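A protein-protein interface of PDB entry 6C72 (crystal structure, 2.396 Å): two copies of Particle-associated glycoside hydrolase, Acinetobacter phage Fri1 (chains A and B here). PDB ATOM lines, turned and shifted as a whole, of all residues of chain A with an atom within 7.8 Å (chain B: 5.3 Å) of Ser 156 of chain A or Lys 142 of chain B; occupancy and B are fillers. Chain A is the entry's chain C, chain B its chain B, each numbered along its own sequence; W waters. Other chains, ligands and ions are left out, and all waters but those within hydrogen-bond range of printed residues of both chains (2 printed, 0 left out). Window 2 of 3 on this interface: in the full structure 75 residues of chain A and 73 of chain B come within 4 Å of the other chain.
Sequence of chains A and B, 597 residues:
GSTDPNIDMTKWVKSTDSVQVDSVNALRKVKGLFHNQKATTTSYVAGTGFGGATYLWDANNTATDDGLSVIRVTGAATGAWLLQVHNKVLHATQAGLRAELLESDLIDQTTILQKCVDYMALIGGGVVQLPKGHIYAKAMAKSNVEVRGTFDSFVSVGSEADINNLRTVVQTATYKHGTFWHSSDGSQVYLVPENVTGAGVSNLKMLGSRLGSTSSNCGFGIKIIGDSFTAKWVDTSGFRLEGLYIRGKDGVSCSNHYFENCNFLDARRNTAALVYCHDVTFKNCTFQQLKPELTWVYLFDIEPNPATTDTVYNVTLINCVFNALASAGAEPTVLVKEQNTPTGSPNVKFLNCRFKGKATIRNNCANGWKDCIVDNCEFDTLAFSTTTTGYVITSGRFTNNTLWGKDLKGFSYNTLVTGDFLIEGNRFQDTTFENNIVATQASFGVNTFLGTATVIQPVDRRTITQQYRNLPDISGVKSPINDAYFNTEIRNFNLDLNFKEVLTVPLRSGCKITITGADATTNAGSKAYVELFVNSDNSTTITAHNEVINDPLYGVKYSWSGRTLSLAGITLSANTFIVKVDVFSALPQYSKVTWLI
Of the 13 printed residues of chain B, 4 touch a printed residue of chain A.
Hydrophobic or aromatic side chains of chain B within 4 Å of the printed part of chain A: Ala 121 and Val 196.
Printed residues of chain A that touch a printed residue of chain B: Ser 153, Phe 154, Ser 156 and Gln 171.
Among the printed residues, no Asp or Glu carboxylate lies within 4 Å of a Lys or Arg side-chain nitrogen of the other chain.
Ser 153 of chain A touches Ala 121 of chain B (CA to O, 3.6 Å).
Phe 154 of chain A touches Lys 142 of chain B (CE2 to CD, 3.9 Å).
Phe 154 of chain A touches Ser 143 of chain B.
Gln 171 of chain A touches Val 196 of chain B (NE2 to CG2, 3.9 Å).
The side-chain amino group (NZ) of Lys 142 of chain B lies within hydrogen-bond range of the side-chain hydroxyl (OG) of Ser 156 of chain A (2.7 Å).
N of Phe 154 of chain A lies within hydrogen-bond range of O of Ala 121 of chain B.
The backbone NH (N) of Val 157 of chain A lies within hydrogen-bond range of the side-chain amide oxygen (OE1) of Gln 171 of chain A, at 3.0 Å.
The side-chain hydroxyl (OG) of Ser 143 of chain B sits at hydrogen-bond distance from the backbone NH (N) of Thr 197 of chain B (3.0 Å).
The side-chain carboxylate of Asp 118 of chain B is in salt-bridge range of the side-chain amino group of Lys 142 of chain B (2.8 Å).
The side-chain amide nitrogen (NE2) of Gln 171 of chain A lies within hydrogen-bond range of the backbone carbonyl oxygen (O) of Ala 173 of chain A (2.9 Å).
No position is printed for both chains.
Of the printed residues of chain B, Ser 156 of chain A touches Lys 142 (2.7 Å).
Ser 159 of chain A touches none of the printed residues of chain B.
Printed residues of chain B within 4 Å of Gln 171 of chain A: Val 196 (3.9 Å).
Asp 118 of chain B touches none of the printed residues of chain A.
Of the printed residues of chain A, Ala 121 of chain B touches Ser 153 (3.6 Å) and Phe 154 (2.9 Å).
Ala 141 of chain B touches none of the printed residues of chain A.
Of chain A, only Phe 154 (3.9 Å) and Ser 156 (2.7 Å) come within 4 Å of Lys 142 of chain B.
The nearest residue of chain B that does not touch Ser 156 of chain A is Met 140 of chain B (4.4 Å).
The nearest printed residue of chain A that does not touch Ala 121 of chain B is Val 155 of chain A (5.5 Å).
Water W2 lies within hydrogen-bond range of O of Phe 154 of chain A (2.6 Å) and O of Asp 118 of chain B (2.8 Å).
Water W1 lies within hydrogen-bond range of NZ of Lys 142 of chain B (2.7 Å) and N of Ser 156 of chain A (2.9 Å).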
ATOM      1  N   SER A 153     -11.312  -4.768  21.604  1.00  0.00           N
ATOM      2  CA  SER A 153     -12.148  -4.755  20.409  1.00  0.00           C
ATOM      3  C   SER A 153     -13.547  -4.221  20.718  1.00  0.00           C
ATOM      4  O   SER A 153     -14.130  -4.502  21.769  1.00  0.00           O
ATOM      5  CB  SER A 153     -12.250  -6.158  19.816  1.00  0.00           C
ATOM      6  OG  SER A 153     -12.948  -7.005  20.705  1.00  0.00           O
ATOM      7  N   PHE A 154     -14.096  -3.463  19.777  1.00  0.00           N
ATOM      8  CA  PHE A 154     -15.454  -2.955  19.870  1.00  0.00           C
ATOM      9  C   PHE A 154     -16.278  -3.606  18.765  1.00  0.00           C
ATOM     10  O   PHE A 154     -15.952  -3.471  17.579  1.00  0.00           O
ATOM     11  CB  PHE A 154     -15.484  -1.433  19.746  1.00  0.00           C
ATOM     12  CG  PHE A 154     -16.859  -0.858  19.888  1.00  0.00           C
ATOM     13  CD1 PHE A 154     -17.380  -0.602  21.150  1.00  0.00           C
ATOM     14  CD2 PHE A 154     -17.643  -0.617  18.771  1.00  0.00           C
ATOM     15  CE1 PHE A 154     -18.651  -0.097  21.299  1.00  0.00           C
ATOM     16  CE2 PHE A 154     -18.917  -0.114  18.902  1.00  0.00           C
ATOM     17  CZ  PHE A 154     -19.429   0.156  20.174  1.00  0.00           C
ATOM     18  N   VAL A 155     -17.332  -4.323  19.149  1.00  0.00           N
ATOM     19  CA  VAL A 155     -18.238  -4.956  18.195  1.00  0.00           C
ATOM     20  C   VAL A 155     -19.635  -4.458  18.517  1.00  0.00           C
ATOM     21  O   VAL A 155     -20.179  -4.771  19.585  1.00  0.00           O
ATOM     22  CB  VAL A 155     -18.169  -6.490  18.249  1.00  0.00           C
ATOM     23  CG1 VAL A 155     -19.191  -7.103  17.294  1.00  0.00           C
ATOM     24  CG2 VAL A 155     -16.761  -6.974  17.914  1.00  0.00           C
ATOM     25  N   SER A 156     -20.217  -3.678  17.609  1.00  0.00           N
ATOM     26  CA  SER A 156     -21.521  -3.096  17.891  1.00  0.00           C
ATOM     27  C   SER A 156     -22.599  -4.164  17.838  1.00  0.00           C
ATOM     28  O   SER A 156     -22.421  -5.236  17.255  1.00  0.00           O
ATOM     29  CB  SER A 156     -21.858  -1.981  16.905  1.00  0.00           C
ATOM     30  OG  SER A 156     -22.023  -2.492  15.603  1.00  0.00           O
ATOM     31  N   VAL A 157     -23.729  -3.851  18.460  1.00  0.00           N
ATOM     32  CA  VAL A 157     -24.905  -4.708  18.481  1.00  0.00           C
ATOM     33  C   VAL A 157     -26.064  -3.931  17.869  1.00  0.00           C
ATOM     34  O   VAL A 157     -26.151  -2.710  18.030  1.00  0.00           O
ATOM     35  CB  VAL A 157     -25.213  -5.170  19.922  1.00  0.00           C
ATOM     36  CG1 VAL A 157     -26.563  -5.863  20.021  1.00  0.00           C
ATOM     37  CG2 VAL A 157     -24.127  -6.129  20.397  1.00  0.00           C
ATOM     38  N   GLY A 158     -26.916  -4.625  17.128  1.00  0.00           N
ATOM     39  CA  GLY A 158     -28.172  -4.080  16.649  1.00  0.00           C
ATOM     40  C   GLY A 158     -28.117  -3.616  15.203  1.00  0.00           C
ATOM     41  O   GLY A 158     -27.080  -3.171  14.696  1.00  0.00           O
ATOM     42  N   SER A 159     -29.269  -3.663  14.544  1.00  0.00           N
ATOM     43  CA  SER A 159     -29.363  -3.250  13.156  1.00  0.00           C
ATOM     44  C   SER A 159     -29.525  -1.741  13.059  1.00  0.00           C
ATOM     45  O   SER A 159     -29.989  -1.076  13.992  1.00  0.00           O
ATOM     46  CB  SER A 159     -30.551  -3.919  12.475  1.00  0.00           C
ATOM     47  OG  SER A 159     -31.769  -3.399  12.997  1.00  0.00           O
ATOM     48  N   ILE A 163     -31.759   0.775  15.514  1.00  0.00           N
ATOM     49  CA  ILE A 163     -31.097   1.913  16.146  1.00  0.00           C
ATOM     50  C   ILE A 163     -31.810   3.212  15.790  1.00  0.00           C
ATOM     51  O   ILE A 163     -31.963   4.107  16.635  1.00  0.00           O
ATOM     52  CB  ILE A 163     -29.609   1.943  15.750  1.00  0.00           C
ATOM     53  CG1 ILE A 163     -28.873   0.753  16.377  1.00  0.00           C
ATOM     54  CG2 ILE A 163     -28.942   3.244  16.153  1.00  0.00           C
ATOM     55  CD1 ILE A 163     -27.433   0.620  15.922  1.00  0.00           C
ATOM     56  N   VAL A 170     -30.592   0.295  21.618  1.00  0.00           N
ATOM     57  CA  VAL A 170     -30.393  -0.910  20.825  1.00  0.00           C
ATOM     58  C   VAL A 170     -28.915  -1.278  20.746  1.00  0.00           C
ATOM     59  O   VAL A 170     -28.538  -2.438  20.935  1.00  0.00           O
ATOM     60  CB  VAL A 170     -30.998  -0.746  19.410  1.00  0.00           C
ATOM     61  CG1 VAL A 170     -30.721  -1.980  18.566  1.00  0.00           C
ATOM     62  CG2 VAL A 170     -32.495  -0.459  19.488  1.00  0.00           C
ATOM     63  N   GLN A 171     -28.063  -0.296  20.467  1.00  0.00           N
ATOM     64  CA  GLN A 171     -26.625  -0.529  20.410  1.00  0.00           C
ATOM     65  C   GLN A 171     -26.112  -0.497  21.844  1.00  0.00           C
ATOM     66  O   GLN A 171     -25.836   0.566  22.399  1.00  0.00           O
ATOM     67  CB  GLN A 171     -25.954   0.515  19.520  1.00  0.00           C
ATOM     68  CG  GLN A 171     -24.636   0.074  18.930  1.00  0.00           C
ATOM     69  CD  GLN A 171     -23.619  -0.291  19.987  1.00  0.00           C
ATOM     70  OE1 GLN A 171     -23.375  -1.471  20.249  1.00  0.00           O
ATOM     71  NE2 GLN A 171     -23.019   0.720  20.603  1.00  0.00           N
ATOM     72  N   THR A 172     -25.951  -1.678  22.430  1.00  0.00           N
ATOM     73  CA  THR A 172     -25.646  -1.825  23.845  1.00  0.00           C
ATOM     74  C   THR A 172     -24.161  -1.996  24.139  1.00  0.00           C
ATOM     75  O   THR A 172     -23.775  -1.943  25.311  1.00  0.00           O
ATOM     76  CB  THR A 172     -26.427  -3.013  24.415  1.00  0.00           C
ATOM     77  OG1 THR A 172     -26.178  -4.170  23.611  1.00  0.00           O
ATOM     78  CG2 THR A 172     -27.930  -2.718  24.428  1.00  0.00           C
ATOM     79  N   ALA A 173     -23.326  -2.182  23.119  1.00  0.00           N
ATOM     80  CA  ALA A 173     -21.899  -2.380  23.317  1.00  0.00           C
ATOM     81  C   ALA A 173     -21.216  -1.054  23.622  1.00  0.00           C
ATOM     82  O   ALA A 173     -21.535  -0.023  23.027  1.00  0.00           O
ATOM     83  CB  ALA A 173     -21.274  -3.015  22.077  1.00  0.00           C
ATOM     84  N   THR A 174     -20.287  -1.078  24.571  1.00  0.00           N
ATOM     85  CA  THR A 174     -19.527   0.103  24.958  1.00  0.00           C
ATOM     86  C   THR A 174     -18.039  -0.199  24.881  1.00  0.00           C
ATOM     87  O   THR A 174     -17.618  -1.346  25.047  1.00  0.00           O
ATOM     88  CB  THR A 174     -19.896   0.571  26.392  1.00  0.00           C
ATOM     89  OG1 THR A 174     -19.694  -0.509  27.310  1.00  0.00           O
ATOM     90  CG2 THR A 174     -21.335   1.025  26.467  1.00  0.00           C
ATOM     91  N   GLN B 114     -18.168  -0.328   5.436  1.00  0.00           N
ATOM     92  CA  GLN B 114     -18.514  -0.793   6.773  1.00  0.00           C
ATOM     93  C   GLN B 114     -17.523  -1.836   7.269  1.00  0.00           C
ATOM     94  O   GLN B 114     -17.197  -1.869   8.463  1.00  0.00           O
ATOM     95  CB  GLN B 114     -19.942  -1.335   6.801  1.00  0.00           C
ATOM     96  CG  GLN B 114     -20.474  -1.536   8.209  1.00  0.00           C
ATOM     97  CD  GLN B 114     -20.459  -0.249   9.011  1.00  0.00           C
ATOM     98  OE1 GLN B 114     -21.070   0.741   8.618  1.00  0.00           O
ATOM     99  NE2 GLN B 114     -19.785  -0.263  10.151  1.00  0.00           N
ATOM    100  N   VAL B 117     -14.585   0.096   8.769  1.00  0.00           N
ATOM    101  CA  VAL B 117     -14.900   0.684  10.070  1.00  0.00           C
ATOM    102  C   VAL B 117     -15.008  -0.401  11.136  1.00  0.00           C
ATOM    103  O   VAL B 117     -14.436  -0.283  12.225  1.00  0.00           O
ATOM    104  CB  VAL B 117     -16.187   1.523   9.984  1.00  0.00           C
ATOM    105  CG1 VAL B 117     -16.604   1.977  11.369  1.00  0.00           C
ATOM    106  CG2 VAL B 117     -15.963   2.730   9.086  1.00  0.00           C
ATOM    107  N   ASP B 118     -15.713  -1.490  10.823  1.00  0.00           N
ATOM    108  CA  ASP B 118     -15.850  -2.579  11.782  1.00  0.00           C
ATOM    109  C   ASP B 118     -14.502  -3.185  12.129  1.00  0.00           C
ATOM    110  O   ASP B 118     -14.239  -3.503  13.296  1.00  0.00           O
ATOM    111  CB  ASP B 118     -16.771  -3.655  11.227  1.00  0.00           C
ATOM    112  CG  ASP B 118     -18.196  -3.212  11.208  1.00  0.00           C
ATOM    113  OD1 ASP B 118     -18.441  -2.078  11.660  1.00  0.00           O
ATOM    114  OD2 ASP B 118     -19.058  -3.971  10.723  1.00  0.00           O
ATOM    115  N   ALA B 121     -12.374  -0.883  14.413  1.00  0.00           N
ATOM    116  CA  ALA B 121     -12.885  -0.976  15.773  1.00  0.00           C
ATOM    117  C   ALA B 121     -12.530  -2.307  16.417  1.00  0.00           C
ATOM    118  O   ALA B 121     -12.455  -2.392  17.647  1.00  0.00           O
ATOM    119  CB  ALA B 121     -14.401  -0.764  15.794  1.00  0.00           C
ATOM    120  N   MET B 140     -21.969   3.016   9.504  1.00  0.00           N
ATOM    121  CA  MET B 140     -22.276   3.084  10.919  1.00  0.00           C
ATOM    122  C   MET B 140     -20.970   3.306  11.673  1.00  0.00           C
ATOM    123  O   MET B 140     -20.067   2.464  11.622  1.00  0.00           O
ATOM    124  CB  MET B 140     -22.964   1.795  11.360  1.00  0.00           C
ATOM    125  CG  MET B 140     -23.392   1.762  12.812  1.00  0.00           C
ATOM    126  SD  MET B 140     -24.362   0.289  13.207  1.00  0.00           S
ATOM    127  CE  MET B 140     -25.596   0.356  11.909  1.00  0.00           C
ATOM    128  N   ALA B 141     -20.866   4.431  12.370  1.00  0.00           N
ATOM    129  CA  ALA B 141     -19.658   4.715  13.133  1.00  0.00           C
ATOM    130  C   ALA B 141     -19.466   3.686  14.246  1.00  0.00           C
ATOM    131  O   ALA B 141     -20.424   3.110  14.764  1.00  0.00           O
ATOM    132  CB  ALA B 141     -19.717   6.117  13.736  1.00  0.00           C
ATOM    133  N   LYS B 142     -18.206   3.431  14.578  1.00  0.00           N
ATOM    134  CA  LYS B 142     -17.833   2.554  15.674  1.00  0.00           C
ATOM    135  C   LYS B 142     -16.849   3.302  16.554  1.00  0.00           C
ATOM    136  O   LYS B 142     -16.223   4.274  16.125  1.00  0.00           O
ATOM    137  CB  LYS B 142     -17.230   1.233  15.180  1.00  0.00           C
ATOM    138  CG  LYS B 142     -18.172   0.413  14.311  1.00  0.00           C
ATOM    139  CD  LYS B 142     -19.477   0.165  15.041  1.00  0.00           C
ATOM    140  CE  LYS B 142     -20.579  -0.241  14.077  1.00  0.00           C
ATOM    141  NZ  LYS B 142     -20.455  -1.660  13.627  1.00  0.00           N
ATOM    142  N   SER B 143     -16.744   2.857  17.805  1.00  0.00           N
ATOM    143  CA  SER B 143     -16.034   3.634  18.814  1.00  0.00           C
ATOM    144  C   SER B 143     -14.554   3.803  18.471  1.00  0.00           C
ATOM    145  O   SER B 143     -13.871   2.853  18.070  1.00  0.00           O
ATOM    146  CB  SER B 143     -16.198   2.976  20.185  1.00  0.00           C
ATOM    147  OG  SER B 143     -17.556   3.045  20.606  1.00  0.00           O
ATOM    148  N   ASN B 144     -14.062   5.032  18.647  1.00  0.00           N
ATOM    149  CA  ASN B 144     -12.649   5.374  18.473  1.00  0.00           C
ATOM    150  C   ASN B 144     -12.167   5.170  17.038  1.00  0.00           C
ATOM    151  O   ASN B 144     -10.966   5.025  16.797  1.00  0.00           O
ATOM    152  CB  ASN B 144     -11.782   4.576  19.445  1.00  0.00           C
ATOM    153  CG  ASN B 144     -12.227   4.759  20.872  1.00  0.00           C
ATOM    154  OD1 ASN B 144     -12.364   5.896  21.336  1.00  0.00           O
ATOM    155  ND2 ASN B 144     -12.503   3.652  21.567  1.00  0.00           N
ATOM    156  N   VAL B 145     -13.082   5.248  16.075  1.00  0.00           N
ATOM    157  CA  VAL B 145     -12.758   5.177  14.657  1.00  0.00           C
ATOM    158  C   VAL B 145     -13.120   6.511  14.025  1.00  0.00           C
ATOM    159  O   VAL B 145     -14.191   7.066  14.308  1.00  0.00           O
ATOM    160  CB  VAL B 145     -13.507   4.036  13.948  1.00  0.00           C
ATOM    161  CG1 VAL B 145     -13.293   4.128  12.454  1.00  0.00           C
ATOM    162  CG2 VAL B 145     -13.057   2.679  14.497  1.00  0.00           C
ATOM    163  N   VAL B 196     -21.628   4.454  21.021  1.00  0.00           N
ATOM    164  CA  VAL B 196     -20.427   4.586  20.209  1.00  0.00           C
ATOM    165  C   VAL B 196     -19.760   5.890  20.620  1.00  0.00           C
ATOM    166  O   VAL B 196     -20.347   6.965  20.469  1.00  0.00           O
ATOM    167  CB  VAL B 196     -20.767   4.587  18.706  1.00  0.00           C
ATOM    168  CG1 VAL B 196     -19.565   5.005  17.885  1.00  0.00           C
ATOM    169  CG2 VAL B 196     -21.264   3.225  18.264  1.00  0.00           C
ATOM    170  N   THR B 197     -18.532   5.804  21.118  1.00  0.00           N
ATOM    171  CA  THR B 197     -17.855   6.934  21.733  1.00  0.00           C
ATOM    172  C   THR B 197     -16.570   7.266  20.988  1.00  0.00           C
ATOM    173  O   THR B 197     -15.882   6.379  20.463  1.00  0.00           O
ATOM    174  CB  THR B 197     -17.507   6.638  23.190  1.00  0.00           C
ATOM    175  OG1 THR B 197     -16.714   5.442  23.244  1.00  0.00           O
ATOM    176  CG2 THR B 197     -18.773   6.444  24.025  1.00  0.00           C
ATOM    177  N   ALA B 199     -15.858   8.615  18.172  1.00  0.00           N
ATOM    178  CA  ALA B 199     -15.797   8.525  16.721  1.00  0.00           C
ATOM    179  C   ALA B 199     -15.617   9.918  16.118  1.00  0.00           C
ATOM    180  O   ALA B 199     -15.667  10.934  16.814  1.00  0.00           O
ATOM    181  CB  ALA B 199     -17.049   7.847  16.164  1.00  0.00           C
HETATM  182  O   HOH W   1     -18.965  -3.520  14.994  1.00  0.00           O
HETATM  183  O   HOH W   2     -16.258  -4.295  15.111  1.00  0.00           O
